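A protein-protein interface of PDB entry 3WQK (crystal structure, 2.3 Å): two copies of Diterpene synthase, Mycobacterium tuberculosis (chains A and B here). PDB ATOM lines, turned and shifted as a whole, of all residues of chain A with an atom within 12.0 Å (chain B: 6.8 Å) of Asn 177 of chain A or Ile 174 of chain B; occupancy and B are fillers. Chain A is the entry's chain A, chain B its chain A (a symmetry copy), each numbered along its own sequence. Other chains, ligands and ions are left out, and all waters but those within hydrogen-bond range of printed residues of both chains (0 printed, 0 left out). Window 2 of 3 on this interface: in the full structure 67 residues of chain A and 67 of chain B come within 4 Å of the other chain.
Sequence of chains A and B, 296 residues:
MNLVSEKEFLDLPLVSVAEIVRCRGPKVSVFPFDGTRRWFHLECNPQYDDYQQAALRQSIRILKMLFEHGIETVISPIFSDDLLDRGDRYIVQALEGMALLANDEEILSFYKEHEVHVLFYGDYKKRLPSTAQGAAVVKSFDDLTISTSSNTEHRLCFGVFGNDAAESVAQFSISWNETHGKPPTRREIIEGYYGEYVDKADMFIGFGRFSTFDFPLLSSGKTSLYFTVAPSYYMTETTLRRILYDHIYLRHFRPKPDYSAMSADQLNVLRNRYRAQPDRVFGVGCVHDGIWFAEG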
ATOM      1  N   ALA A 166      -1.912  -8.787  16.053  1.00  0.00           N
ATOM      2  CA  ALA A 166      -1.036  -9.320  17.114  1.00  0.00           C
ATOM      3  C   ALA A 166      -1.534  -9.131  18.562  1.00  0.00           C
ATOM      4  O   ALA A 166      -1.852 -10.103  19.242  1.00  0.00           O
ATOM      5  CB  ALA A 166       0.384  -8.741  16.967  1.00  0.00           C
ATOM      6  N   GLU A 167      -1.602  -7.886  19.027  1.00  0.00           N
ATOM      7  CA  GLU A 167      -2.059  -7.614  20.383  1.00  0.00           C
ATOM      8  C   GLU A 167      -3.428  -8.228  20.646  1.00  0.00           C
ATOM      9  O   GLU A 167      -3.703  -8.702  21.745  1.00  0.00           O
ATOM     10  CB  GLU A 167      -2.108  -6.104  20.636  1.00  0.00           C
ATOM     11  CG  GLU A 167      -2.355  -5.725  22.098  1.00  0.00           C
ATOM     12  CD  GLU A 167      -1.450  -6.491  23.070  1.00  0.00           C
ATOM     13  OE1 GLU A 167      -0.246  -6.616  22.791  1.00  0.00           O
ATOM     14  OE2 GLU A 167      -1.940  -6.966  24.113  1.00  0.00           O
ATOM     15  N   SER A 168      -4.286  -8.221  19.629  1.00  0.00           N
ATOM     16  CA  SER A 168      -5.628  -8.779  19.748  1.00  0.00           C
ATOM     17  C   SER A 168      -5.598 -10.299  19.913  1.00  0.00           C
ATOM     18  O   SER A 168      -6.379 -10.873  20.685  1.00  0.00           O
ATOM     19  CB  SER A 168      -6.457  -8.418  18.518  1.00  0.00           C
ATOM     20  OG  SER A 168      -7.674  -9.132  18.536  1.00  0.00           O
ATOM     21  N   VAL A 169      -4.711 -10.953  19.172  1.00  0.00           N
ATOM     22  CA  VAL A 169      -4.566 -12.401  19.285  1.00  0.00           C
ATOM     23  C   VAL A 169      -4.030 -12.757  20.680  1.00  0.00           C
ATOM     24  O   VAL A 169      -4.504 -13.697  21.313  1.00  0.00           O
ATOM     25  CB  VAL A 169      -3.586 -12.962  18.221  1.00  0.00           C
ATOM     26  CG1 VAL A 169      -3.275 -14.426  18.521  1.00  0.00           C
ATOM     27  CG2 VAL A 169      -4.191 -12.833  16.845  1.00  0.00           C
ATOM     28  N   ALA A 170      -3.039 -11.997  21.143  1.00  0.00           N
ATOM     29  CA  ALA A 170      -2.441 -12.226  22.451  1.00  0.00           C
ATOM     30  C   ALA A 170      -3.512 -12.186  23.541  1.00  0.00           C
ATOM     31  O   ALA A 170      -3.681 -13.140  24.300  1.00  0.00           O
ATOM     32  CB  ALA A 170      -1.372 -11.168  22.734  1.00  0.00           C
ATOM     33  N   GLN A 171      -4.251 -11.084  23.600  1.00  0.00           N
ATOM     34  CA  GLN A 171      -5.282 -10.927  24.616  1.00  0.00           C
ATOM     35  C   GLN A 171      -6.412 -11.928  24.455  1.00  0.00           C
ATOM     36  O   GLN A 171      -6.932 -12.441  25.445  1.00  0.00           O
ATOM     37  CB  GLN A 171      -5.797  -9.482  24.616  1.00  0.00           C
ATOM     38  CG  GLN A 171      -4.680  -8.482  24.953  1.00  0.00           C
ATOM     39  CD  GLN A 171      -5.172  -7.056  25.135  1.00  0.00           C
ATOM     40  OE1 GLN A 171      -4.375  -6.126  25.288  1.00  0.00           O
ATOM     41  NE2 GLN A 171      -6.489  -6.876  25.123  1.00  0.00           N
ATOM     42  N   PHE A 172      -6.791 -12.228  23.218  1.00  0.00           N
ATOM     43  CA  PHE A 172      -7.838 -13.221  23.001  1.00  0.00           C
ATOM     44  C   PHE A 172      -7.347 -14.586  23.508  1.00  0.00           C
ATOM     45  O   PHE A 172      -8.109 -15.359  24.089  1.00  0.00           O
ATOM     46  CB  PHE A 172      -8.169 -13.354  21.519  1.00  0.00           C
ATOM     47  CG  PHE A 172      -8.963 -14.592  21.194  1.00  0.00           C
ATOM     48  CD1 PHE A 172     -10.352 -14.585  21.260  1.00  0.00           C
ATOM     49  CD2 PHE A 172      -8.314 -15.772  20.838  1.00  0.00           C
ATOM     50  CE1 PHE A 172     -11.080 -15.728  20.975  1.00  0.00           C
ATOM     51  CE2 PHE A 172      -9.035 -16.926  20.549  1.00  0.00           C
ATOM     52  CZ  PHE A 172     -10.421 -16.908  20.616  1.00  0.00           C
ATOM     53  N   SER A 173      -6.074 -14.877  23.262  1.00  0.00           N
ATOM     54  CA  SER A 173      -5.482 -16.148  23.673  1.00  0.00           C
ATOM     55  C   SER A 173      -5.360 -16.251  25.189  1.00  0.00           C
ATOM     56  O   SER A 173      -5.626 -17.301  25.771  1.00  0.00           O
ATOM     57  CB  SER A 173      -4.106 -16.330  23.020  1.00  0.00           C
ATOM     58  OG  SER A 173      -4.247 -16.456  21.612  1.00  0.00           O
ATOM     59  N   ILE A 174      -4.965 -15.159  25.829  1.00  0.00           N
ATOM     60  CA  ILE A 174      -4.839 -15.172  27.273  1.00  0.00           C
ATOM     61  C   ILE A 174      -6.188 -15.447  27.940  1.00  0.00           C
ATOM     62  O   ILE A 174      -6.273 -16.279  28.849  1.00  0.00           O
ATOM     63  CB  ILE A 174      -4.239 -13.852  27.775  1.00  0.00           C
ATOM     64  CG1 ILE A 174      -2.754 -13.801  27.370  1.00  0.00           C
ATOM     65  CG2 ILE A 174      -4.440 -13.720  29.286  1.00  0.00           C
ATOM     66  CD1 ILE A 174      -2.055 -12.510  27.704  1.00  0.00           C
ATOM     67  N   SER A 175      -7.246 -14.781  27.486  1.00  0.00           N
ATOM     68  CA  SER A 175      -8.567 -15.007  28.069  1.00  0.00           C
ATOM     69  C   SER A 175      -9.027 -16.440  27.825  1.00  0.00           C
ATOM     70  O   SER A 175      -9.480 -17.120  28.739  1.00  0.00           O
ATOM     71  CB  SER A 175      -9.600 -14.050  27.468  1.00  0.00           C
ATOM     72  OG  SER A 175      -9.214 -12.700  27.659  1.00  0.00           O
ATOM     73  N   TRP A 176      -8.906 -16.893  26.582  1.00  0.00           N
ATOM     74  CA  TRP A 176      -9.333 -18.235  26.220  1.00  0.00           C
ATOM     75  C   TRP A 176      -8.687 -19.320  27.084  1.00  0.00           C
ATOM     76  O   TRP A 176      -9.338 -20.296  27.456  1.00  0.00           O
ATOM     77  CB  TRP A 176      -9.033 -18.492  24.736  1.00  0.00           C
ATOM     78  CG  TRP A 176      -9.489 -19.826  24.245  1.00  0.00           C
ATOM     79  CD1 TRP A 176      -8.901 -21.032  24.488  1.00  0.00           C
ATOM     80  CD2 TRP A 176     -10.647 -20.095  23.444  1.00  0.00           C
ATOM     81  NE1 TRP A 176      -9.622 -22.036  23.891  1.00  0.00           N
ATOM     82  CE2 TRP A 176     -10.700 -21.491  23.246  1.00  0.00           C
ATOM     83  CE3 TRP A 176     -11.651 -19.292  22.882  1.00  0.00           C
ATOM     84  CZ2 TRP A 176     -11.715 -22.107  22.498  1.00  0.00           C
ATOM     85  CZ3 TRP A 176     -12.664 -19.905  22.134  1.00  0.00           C
ATOM     86  CH2 TRP A 176     -12.686 -21.297  21.953  1.00  0.00           C
ATOM     87  N   ASN A 177      -7.408 -19.148  27.399  1.00  0.00           N
ATOM     88  CA  ASN A 177      -6.699 -20.137  28.203  1.00  0.00           C
ATOM     89  C   ASN A 177      -7.130 -20.073  29.664  1.00  0.00           C
ATOM     90  O   ASN A 177      -7.159 -21.086  30.356  1.00  0.00           O
ATOM     91  CB  ASN A 177      -5.187 -19.925  28.094  1.00  0.00           C
ATOM     92  CG  ASN A 177      -4.405 -20.878  28.974  1.00  0.00           C
ATOM     93  OD1 ASN A 177      -3.944 -20.507  30.052  1.00  0.00           O
ATOM     94  ND2 ASN A 177      -4.265 -22.122  28.526  1.00  0.00           N
ATOM     95  N   GLU A 178      -7.465 -18.876  30.124  1.00  0.00           N
ATOM     96  CA  GLU A 178      -7.889 -18.690  31.502  1.00  0.00           C
ATOM     97  C   GLU A 178      -9.219 -19.408  31.711  1.00  0.00           C
ATOM     98  O   GLU A 178      -9.416 -20.108  32.710  1.00  0.00           O
ATOM     99  CB  GLU A 178      -8.044 -17.197  31.799  1.00  0.00           C
ATOM    100  CG  GLU A 178      -7.902 -16.825  33.261  1.00  0.00           C
ATOM    101  CD  GLU A 178      -8.963 -17.468  34.131  1.00  0.00           C
ATOM    102  OE1 GLU A 178      -8.650 -18.458  34.842  1.00  0.00           O
ATOM    103  OE2 GLU A 178     -10.115 -16.985  34.089  1.00  0.00           O
ATOM    104  N   THR A 179     -10.119 -19.258  30.741  1.00  0.00           N
ATOM    105  CA  THR A 179     -11.438 -19.870  30.829  1.00  0.00           C
ATOM    106  C   THR A 179     -11.492 -21.317  30.367  1.00  0.00           C
ATOM    107  O   THR A 179     -12.285 -22.098  30.887  1.00  0.00           O
ATOM    108  CB  THR A 179     -12.493 -19.068  30.014  1.00  0.00           C
ATOM    109  OG1 THR A 179     -12.143 -19.089  28.625  1.00  0.00           O
ATOM    110  CG2 THR A 179     -12.560 -17.626  30.495  1.00  0.00           C
ATOM    111  N   HIS A 180     -10.658 -21.680  29.402  1.00  0.00           N
ATOM    112  CA  HIS A 180     -10.671 -23.041  28.871  1.00  0.00           C
ATOM    113  C   HIS A 180      -9.647 -24.000  29.458  1.00  0.00           C
ATOM    114  O   HIS A 180      -9.867 -25.205  29.453  1.00  0.00           O
ATOM    115  CB  HIS A 180     -10.494 -23.028  27.347  1.00  0.00           C
ATOM    116  CG  HIS A 180     -11.671 -22.479  26.604  1.00  0.00           C
ATOM    117  ND1 HIS A 180     -11.899 -21.127  26.459  1.00  0.00           N
ATOM    118  CD2 HIS A 180     -12.683 -23.104  25.956  1.00  0.00           C
ATOM    119  CE1 HIS A 180     -13.001 -20.943  25.752  1.00  0.00           C
ATOM    120  NE2 HIS A 180     -13.495 -22.126  25.436  1.00  0.00           N
ATOM    121  N   GLY A 181      -8.523 -23.473  29.936  1.00  0.00           N
ATOM    122  CA  GLY A 181      -7.503 -24.337  30.504  1.00  0.00           C
ATOM    123  C   GLY A 181      -6.412 -24.683  29.509  1.00  0.00           C
ATOM    124  O   GLY A 181      -5.361 -25.199  29.877  1.00  0.00           O
ATOM    125  N   LYS A 182      -6.662 -24.403  28.238  1.00  0.00           N
ATOM    126  CA  LYS A 182      -5.680 -24.674  27.197  1.00  0.00           C
ATOM    127  C   LYS A 182      -5.679 -23.542  26.186  1.00  0.00           C
ATOM    128  O   LYS A 182      -6.621 -22.744  26.127  1.00  0.00           O
ATOM    129  CB  LYS A 182      -5.984 -25.996  26.477  1.00  0.00           C
ATOM    130  CG  LYS A 182      -7.377 -26.089  25.886  1.00  0.00           C
ATOM    131  CD  LYS A 182      -7.488 -27.191  24.823  1.00  0.00           C
ATOM    132  CE  LYS A 182      -6.669 -26.841  23.575  1.00  0.00           C
ATOM    133  NZ  LYS A 182      -6.998 -27.675  22.370  1.00  0.00           N
ATOM    134  N   PRO A 183      -4.611 -23.449  25.383  1.00  0.00           N
ATOM    135  CA  PRO A 183      -4.521 -22.393  24.372  1.00  0.00           C
ATOM    136  C   PRO A 183      -5.488 -22.679  23.236  1.00  0.00           C
ATOM    137  O   PRO A 183      -5.821 -23.829  22.975  1.00  0.00           O
ATOM    138  CB  PRO A 183      -3.065 -22.474  23.918  1.00  0.00           C
ATOM    139  CG  PRO A 183      -2.762 -23.942  24.049  1.00  0.00           C
ATOM    140  CD  PRO A 183      -3.394 -24.280  25.390  1.00  0.00           C
ATOM    141  N   PRO A 184      -5.981 -21.630  22.565  1.00  0.00           N
ATOM    142  CA  PRO A 184      -6.909 -21.864  21.455  1.00  0.00           C
ATOM    143  C   PRO A 184      -6.157 -22.406  20.241  1.00  0.00           C
ATOM    144  O   PRO A 184      -4.946 -22.230  20.118  1.00  0.00           O
ATOM    145  CB  PRO A 184      -7.485 -20.472  21.186  1.00  0.00           C
ATOM    146  CG  PRO A 184      -6.329 -19.565  21.522  1.00  0.00           C
ATOM    147  CD  PRO A 184      -5.797 -20.186  22.808  1.00  0.00           C
ATOM    148  N   THR A 185      -6.880 -23.075  19.356  1.00  0.00           N
ATOM    149  CA  THR A 185      -6.286 -23.594  18.133  1.00  0.00           C
ATOM    150  C   THR A 185      -6.290 -22.432  17.141  1.00  0.00           C
ATOM    151  O   THR A 185      -6.898 -21.384  17.400  1.00  0.00           O
ATOM    152  CB  THR A 185      -7.138 -24.729  17.526  1.00  0.00           C
ATOM    153  OG1 THR A 185      -8.478 -24.248  17.313  1.00  0.00           O
ATOM    154  CG2 THR A 185      -7.170 -25.949  18.463  1.00  0.00           C
ATOM    155  N   ARG A 186      -5.618 -22.619  16.011  1.00  0.00           N
ATOM    156  CA  ARG A 186      -5.576 -21.587  14.984  1.00  0.00           C
ATOM    157  C   ARG A 186      -7.003 -21.259  14.561  1.00  0.00           C
ATOM    158  O   ARG A 186      -7.368 -20.096  14.380  1.00  0.00           O
ATOM    159  CB  ARG A 186      -4.787 -22.070  13.764  1.00  0.00           C
ATOM    160  CG  ARG A 186      -4.947 -21.143  12.576  1.00  0.00           C
ATOM    161  CD  ARG A 186      -4.014 -21.466  11.427  1.00  0.00           C
ATOM    162  NE  ARG A 186      -4.208 -20.490  10.365  1.00  0.00           N
ATOM    163  CZ  ARG A 186      -5.262 -20.472   9.557  1.00  0.00           C
ATOM    164  NH1 ARG A 186      -6.214 -21.395   9.688  1.00  0.00           N
ATOM    165  NH2 ARG A 186      -5.382 -19.516   8.643  1.00  0.00           N
ATOM    166  N   GLU A 188      -9.777 -21.493  16.282  1.00  0.00           N
ATOM    167  CA  GLU A 188     -10.443 -20.696  17.310  1.00  0.00           C
ATOM    168  C   GLU A 188      -9.894 -19.273  17.348  1.00  0.00           C
ATOM    169  O   GLU A 188     -10.618 -18.325  17.639  1.00  0.00           O
ATOM    170  CB  GLU A 188     -10.286 -21.374  18.680  1.00  0.00           C
ATOM    171  CG  GLU A 188     -11.049 -22.690  18.768  1.00  0.00           C
ATOM    172  CD  GLU A 188     -10.513 -23.644  19.830  1.00  0.00           C
ATOM    173  OE1 GLU A 188     -11.103 -24.735  19.976  1.00  0.00           O
ATOM    174  OE2 GLU A 188      -9.512 -23.315  20.508  1.00  0.00           O
ATOM    175  N   ILE A 189      -8.606 -19.128  17.057  1.00  0.00           N
ATOM    176  CA  ILE A 189      -7.994 -17.806  17.033  1.00  0.00           C
ATOM    177  C   ILE A 189      -8.636 -17.000  15.892  1.00  0.00           C
ATOM    178  O   ILE A 189      -8.973 -15.830  16.055  1.00  0.00           O
ATOM    179  CB  ILE A 189      -6.464 -17.906  16.817  1.00  0.00           C
ATOM    180  CG1 ILE A 189      -5.800 -18.435  18.098  1.00  0.00           C
ATOM    181  CG2 ILE A 189      -5.900 -16.542  16.390  1.00  0.00           C
ATOM    182  CD1 ILE A 189      -4.343 -18.893  17.930  1.00  0.00           C
ATOM    183  N   GLY A 192     -12.112 -16.107  16.706  1.00  0.00           N
ATOM    184  CA  GLY A 192     -12.070 -15.040  17.686  1.00  0.00           C
ATOM    185  C   GLY A 192     -11.856 -13.667  17.077  1.00  0.00           C
ATOM    186  O   GLY A 192     -12.439 -12.677  17.522  1.00  0.00           O
ATOM    187  N   GLU B 167      -0.786 -19.668  16.201  1.00  0.00           N
ATOM    188  CA  GLU B 167      -0.669 -20.563  17.344  1.00  0.00           C
ATOM    189  C   GLU B 167       0.549 -20.226  18.196  1.00  0.00           C
ATOM    190  O   GLU B 167       0.508 -20.332  19.418  1.00  0.00           O
ATOM    191  CB  GLU B 167      -0.590 -22.019  16.876  1.00  0.00           C
ATOM    192  CG  GLU B 167      -0.695 -23.045  18.006  1.00  0.00           C
ATOM    193  CD  GLU B 167      -1.862 -22.758  18.959  1.00  0.00           C
ATOM    194  OE1 GLU B 167      -2.963 -22.444  18.477  1.00  0.00           O
ATOM    195  OE2 GLU B 167      -1.681 -22.850  20.189  1.00  0.00           O
ATOM    196  N   VAL B 169       1.989 -17.216  18.521  1.00  0.00           N
ATOM    197  CA  VAL B 169       1.729 -15.978  19.249  1.00  0.00           C
ATOM    198  C   VAL B 169       0.838 -16.273  20.466  1.00  0.00           C
ATOM    199  O   VAL B 169       1.077 -15.762  21.557  1.00  0.00           O
ATOM    200  CB  VAL B 169       1.014 -14.929  18.356  1.00  0.00           C
ATOM    201  CG1 VAL B 169       0.547 -13.752  19.208  1.00  0.00           C
ATOM    202  CG2 VAL B 169       1.953 -14.446  17.278  1.00  0.00           C
ATOM    203  N   ALA B 170      -0.187 -17.096  20.259  1.00  0.00           N
ATOM    204  CA  ALA B 170      -1.109 -17.459  21.327  1.00  0.00           C
ATOM    205  C   ALA B 170      -0.346 -18.065  22.506  1.00  0.00           C
ATOM    206  O   ALA B 170      -0.434 -17.581  23.634  1.00  0.00           O
ATOM    207  CB  ALA B 170      -2.146 -18.460  20.811  1.00  0.00           C
ATOM    208  N   GLN B 171       0.422 -19.114  22.234  1.00  0.00           N
ATOM    209  CA  GLN B 171       1.172 -19.787  23.285  1.00  0.00           C
ATOM    210  C   GLN B 171       2.241 -18.896  23.894  1.00  0.00           C
ATOM    211  O   GLN B 171       2.462 -18.932  25.103  1.00  0.00           O
ATOM    212  CB  GLN B 171       1.760 -21.097  22.748  1.00  0.00           C
ATOM    213  CG  GLN B 171       0.659 -22.068  22.293  1.00  0.00           C
ATOM    214  CD  GLN B 171       1.178 -23.445  21.913  1.00  0.00           C
ATOM    215  OE1 GLN B 171       0.428 -24.288  21.413  1.00  0.00           O
ATOM    216  NE2 GLN B 171       2.464 -23.681  22.150  1.00  0.00           N
ATOM    217  N   PHE B 172       2.899 -18.084  23.075  1.00  0.00           N
ATOM    218  CA  PHE B 172       3.903 -17.171  23.612  1.00  0.00           C
ATOM    219  C   PHE B 172       3.215 -16.167  24.549  1.00  0.00           C
ATOM    220  O   PHE B 172       3.757 -15.798  25.592  1.00  0.00           O
ATOM    221  CB  PHE B 172       4.587 -16.390  22.496  1.00  0.00           C
ATOM    222  CG  PHE B 172       5.358 -15.195  22.990  1.00  0.00           C
ATOM    223  CD1 PHE B 172       6.683 -15.318  23.392  1.00  0.00           C
ATOM    224  CD2 PHE B 172       4.747 -13.946  23.068  1.00  0.00           C
ATOM    225  CE1 PHE B 172       7.387 -14.221  23.860  1.00  0.00           C
ATOM    226  CE2 PHE B 172       5.444 -12.836  23.536  1.00  0.00           C
ATOM    227  CZ  PHE B 172       6.766 -12.970  23.933  1.00  0.00           C
ATOM    228  N   SER B 173       2.030 -15.715  24.154  1.00  0.00           N
ATOM    229  CA  SER B 173       1.275 -14.743  24.941  1.00  0.00           C
ATOM    230  C   SER B 173       0.769 -15.344  26.248  1.00  0.00           C
ATOM    231  O   SER B 173       0.815 -14.699  27.294  1.00  0.00           O
ATOM    232  CB  SER B 173       0.099 -14.194  24.124  1.00  0.00           C
ATOM    233  OG  SER B 173       0.581 -13.442  23.019  1.00  0.00           O
ATOM    234  N   ILE B 174       0.295 -16.581  26.189  1.00  0.00           N
ATOM    235  CA  ILE B 174      -0.190 -17.227  27.392  1.00  0.00           C
ATOM    236  C   ILE B 174       0.928 -17.376  28.426  1.00  0.00           C
ATOM    237  O   ILE B 174       0.729 -17.065  29.604  1.00  0.00           O
ATOM    238  CB  ILE B 174      -0.813 -18.590  27.060  1.00  0.00           C
ATOM    239  CG1 ILE B 174      -2.143 -18.355  26.318  1.00  0.00           C
ATOM    240  CG2 ILE B 174      -0.991 -19.416  28.335  1.00  0.00           C
ATOM    241  CD1 ILE B 174      -2.820 -19.608  25.831  1.00  0.00           C
ATOM    242  N   SER B 175       2.106 -17.823  27.998  1.00  0.00           N
ATOM    243  CA  SER B 175       3.221 -17.974  28.931  1.00  0.00           C
ATOM    244  C   SER B 175       3.637 -16.623  29.500  1.00  0.00           C
ATOM    245  O   SER B 175       3.802 -16.471  30.705  1.00  0.00           O
ATOM    246  CB  SER B 175       4.430 -18.609  28.238  1.00  0.00           C
ATOM    247  OG  SER B 175       4.094 -19.867  27.681  1.00  0.00           O
ATOM    248  N   TRP B 176       3.803 -15.640  28.621  1.00  0.00           N
ATOM    249  CA  TRP B 176       4.223 -14.313  29.039  1.00  0.00           C
ATOM    250  C   TRP B 176       3.314 -13.710  30.113  1.00  0.00           C
ATOM    251  O   TRP B 176       3.788 -13.059  31.044  1.00  0.00           O
ATOM    252  CB  TRP B 176       4.290 -13.382  27.820  1.00  0.00           C
ATOM    253  CG  TRP B 176       4.771 -12.003  28.133  1.00  0.00           C
ATOM    254  CD1 TRP B 176       4.066 -11.011  28.748  1.00  0.00           C
ATOM    255  CD2 TRP B 176       6.074 -11.468  27.867  1.00  0.00           C
ATOM    256  NE1 TRP B 176       4.850  -9.892  28.884  1.00  0.00           N
ATOM    257  CE2 TRP B 176       6.087 -10.144  28.356  1.00  0.00           C
ATOM    258  CE3 TRP B 176       7.235 -11.983  27.270  1.00  0.00           C
ATOM    259  CZ2 TRP B 176       7.217  -9.317  28.258  1.00  0.00           C
ATOM    260  CZ3 TRP B 176       8.363 -11.158  27.172  1.00  0.00           C
ATOM    261  CH2 TRP B 176       8.343  -9.844  27.665  1.00  0.00           C
ATOM    262  N   ASN B 177       2.010 -13.928  29.980  1.00  0.00           N
ATOM    263  CA  ASN B 177       1.061 -13.379  30.942  1.00  0.00           C
ATOM    264  C   ASN B 177       1.114 -14.137  32.264  1.00  0.00           C
ATOM    265  O   ASN B 177       0.904 -13.562  33.327  1.00  0.00           O
ATOM    266  CB  ASN B 177      -0.358 -13.422  30.372  1.00  0.00           C
ATOM    267  CG  ASN B 177      -1.395 -12.935  31.363  1.00  0.00           C
ATOM    268  OD1 ASN B 177      -2.088 -13.732  31.993  1.00  0.00           O
ATOM    269  ND2 ASN B 177      -1.496 -11.619  31.520  1.00  0.00           N
ATOM    270  N   GLU B 178       1.397 -15.429  32.187  1.00  0.00           N
ATOM    271  CA  GLU B 178       1.472 -16.256  33.380  1.00  0.00           C
ATOM    272  C   GLU B 178       2.659 -15.800  34.224  1.00  0.00           C
ATOM    273  O   GLU B 178       2.553 -15.654  35.446  1.00  0.00           O
ATOM    274  CB  GLU B 178       1.640 -17.724  32.983  1.00  0.00           C
ATOM    275  CG  GLU B 178       1.158 -18.719  34.020  1.00  0.00           C
ATOM    276  CD  GLU B 178       1.924 -18.617  35.324  1.00  0.00           C
ATOM    277  OE1 GLU B 178       1.381 -18.050  36.306  1.00  0.00           O
ATOM    278  OE2 GLU B 178       3.078 -19.098  35.355  1.00  0.00           O
ATOM    279  N   THR B 179       3.781 -15.542  33.557  1.00  0.00           N
ATOM    280  CA  THR B 179       4.994 -15.124  34.245  1.00  0.00           C
ATOM    281  C   THR B 179       5.073 -13.634  34.533  1.00  0.00           C
ATOM    282  O   THR B 179       5.658 -13.232  35.536  1.00  0.00           O
ATOM    283  CB  THR B 179       6.269 -15.524  33.446  1.00  0.00           C
ATOM    284  OG1 THR B 179       6.278 -14.843  32.186  1.00  0.00           O
ATOM    285  CG2 THR B 179       6.303 -17.026  33.207  1.00  0.00           C
ATOM    286  N   PRO B 184       1.692  -9.412  26.653  1.00  0.00           N
ATOM    287  CA  PRO B 184       2.853  -8.751  26.051  1.00  0.00           C
ATOM    288  C   PRO B 184       2.398  -7.664  25.078  1.00  0.00           C
ATOM    289  O   PRO B 184       1.270  -7.687  24.588  1.00  0.00           O
ATOM    290  CB  PRO B 184       3.564  -9.894  25.324  1.00  0.00           C
ATOM    291  CG  PRO B 184       2.420 -10.780  24.901  1.00  0.00           C
ATOM    292  CD  PRO B 184       1.544 -10.790  26.148  1.00  0.00           C
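Among the printed residues, merely in contact across the chains: Ala 170 of chain A with Ser 173 of chain B, Ser 173 of chain A with Ala 170 of chain B, Asn 177 of chain A with Ile 174 of chain B, Ile 174 of chain A with Asn 177 of chain B, Pro 183 of chain A with Ile 174 of chain B, Thr 185 of chain A with Glu 167 of chain B, Arg 186 of chain A with Glu 167 of chain B, Ile 174 of chain A with Ser 173 of chain B, Ser 173 of chain A with Ile 174 of chain B, Ile 189 of chain A with Ala 170 of chain B, Ile 189 of chain A with Glu 167 of chain B, Val 169 of chain A with Val 169 of chain B and Pro 183 of chain A with Glu 167 of chain B.
The side-chain carboxylate (OE2) of Glu 167 of chain A lies close to the side-chain amide oxygen (OE1) of Gln 171 of chain A (2.8 Å).
The backbone carbonyl oxygen (O) of Val 169 of chain A lies within hydrogen-bond range of the side-chain hydroxyl (OG) of Ser 173 of chain A (2.8 Å).
The side-chain amide nitrogen (ND2) of Asn 177 of chain A sits close to the backbone NH (N) of Lys 182 of chain A (3.3 Å).
OE2 of Glu 188 of chain A lies within hydrogen-bond range of N of Thr 185 of chain A, at 2.9 Å.
OE2 of Glu 167 of chain B lies close to OE1 of Gln 171 of chain B.
O of Val 169 of chain B sits at hydrogen-bond distance from OG of Ser 173 of chain B.
Printed residues of chain B within 4 Å of Glu 167 of chain A: Pro 184.
Of the printed residues of chain B, Val 169 of chain A touches Val 169.
Trp 176 of chain A touches none of the printed residues of chain B.
Of the printed residues of chain B, Asn 177 of chain A touches Ile 174.
Of the printed residues of chain B, Pro 184 of chain A touches Glu 167.
Of the printed residues of chain A, Val 169 of chain B touches Val 169 (3.9 Å).
Ala 170 of chain B touches just these residues of chain A: Ser 173 (3.0 Å) and Ile 189 (3.6 Å).
No residue of chain A comes within 4 Å of Glu 178 of chain B.
Printed residues of chain A within 4 Å of Pro 184 of chain B: Glu 167 (2.6 Å).
The nearest residue of chain B that does not touch Asn 177 of chain A is Glu 178 of chain B (6.7 Å).
The nearest printed residue of chain A that does not touch Ile 174 of chain B is Ile 174 of chain A (4.3 Å).
The nearest printed residue of chain A that does not touch Val 169 of chain B is Ala 166 of chain A (4.4 Å).
Hydrophobic or aromatic side chains of chain A within 4 Å of the printed part of chain B: Val 169, Ala 170, Ile 174, Pro 183 and Ile 189.
Of the 13 printed residues of chain B, 7 touch a printed residue of chain A.
Hydrophobic or aromatic side chains of chain B that line the printed part of chain A: Val 169, Ala 170 and Ile 174.
Along chain B the printed residues that touch a printed residue of chain A span positions 167 to 184.
Among the printed residues, no Asp or Glu carboxylate lies within 4 Å of a Lys or Arg side-chain nitrogen of the other chain.
Glu 167 of chain A touches Pro 184 of chain B, and with the chains exchanged Pro 184 of chain A touches Glu 167 of chain B.
Val 169 of chain B touches its own counterpart, Val 169 of chain A.
Ala 170 of chain A touches Ser 173 of chain B, and with the chains exchanged Ser 173 of chain A touches Ala 170 of chain B.
Positions printed for both chains: 167, 169, 170, 171, 172, 173, 174, 175, 176, 177, 178, 179 and 184.
Of the 15 pairs that touch across the chains among the printed residues, 9 have their exchanged pair printed and touching as well.
The side-chain carboxylate (OE1) of Glu 167 of chain A lies close to the backbone carbonyl oxygen (O) of Pro 184 of chain B (2.6 Å).
The backbone carbonyl oxygen (O) of Pro 184 of chain A sits close to the side-chain carboxylate (OE1) of Glu 167 of chain B, 2.6 Å away.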
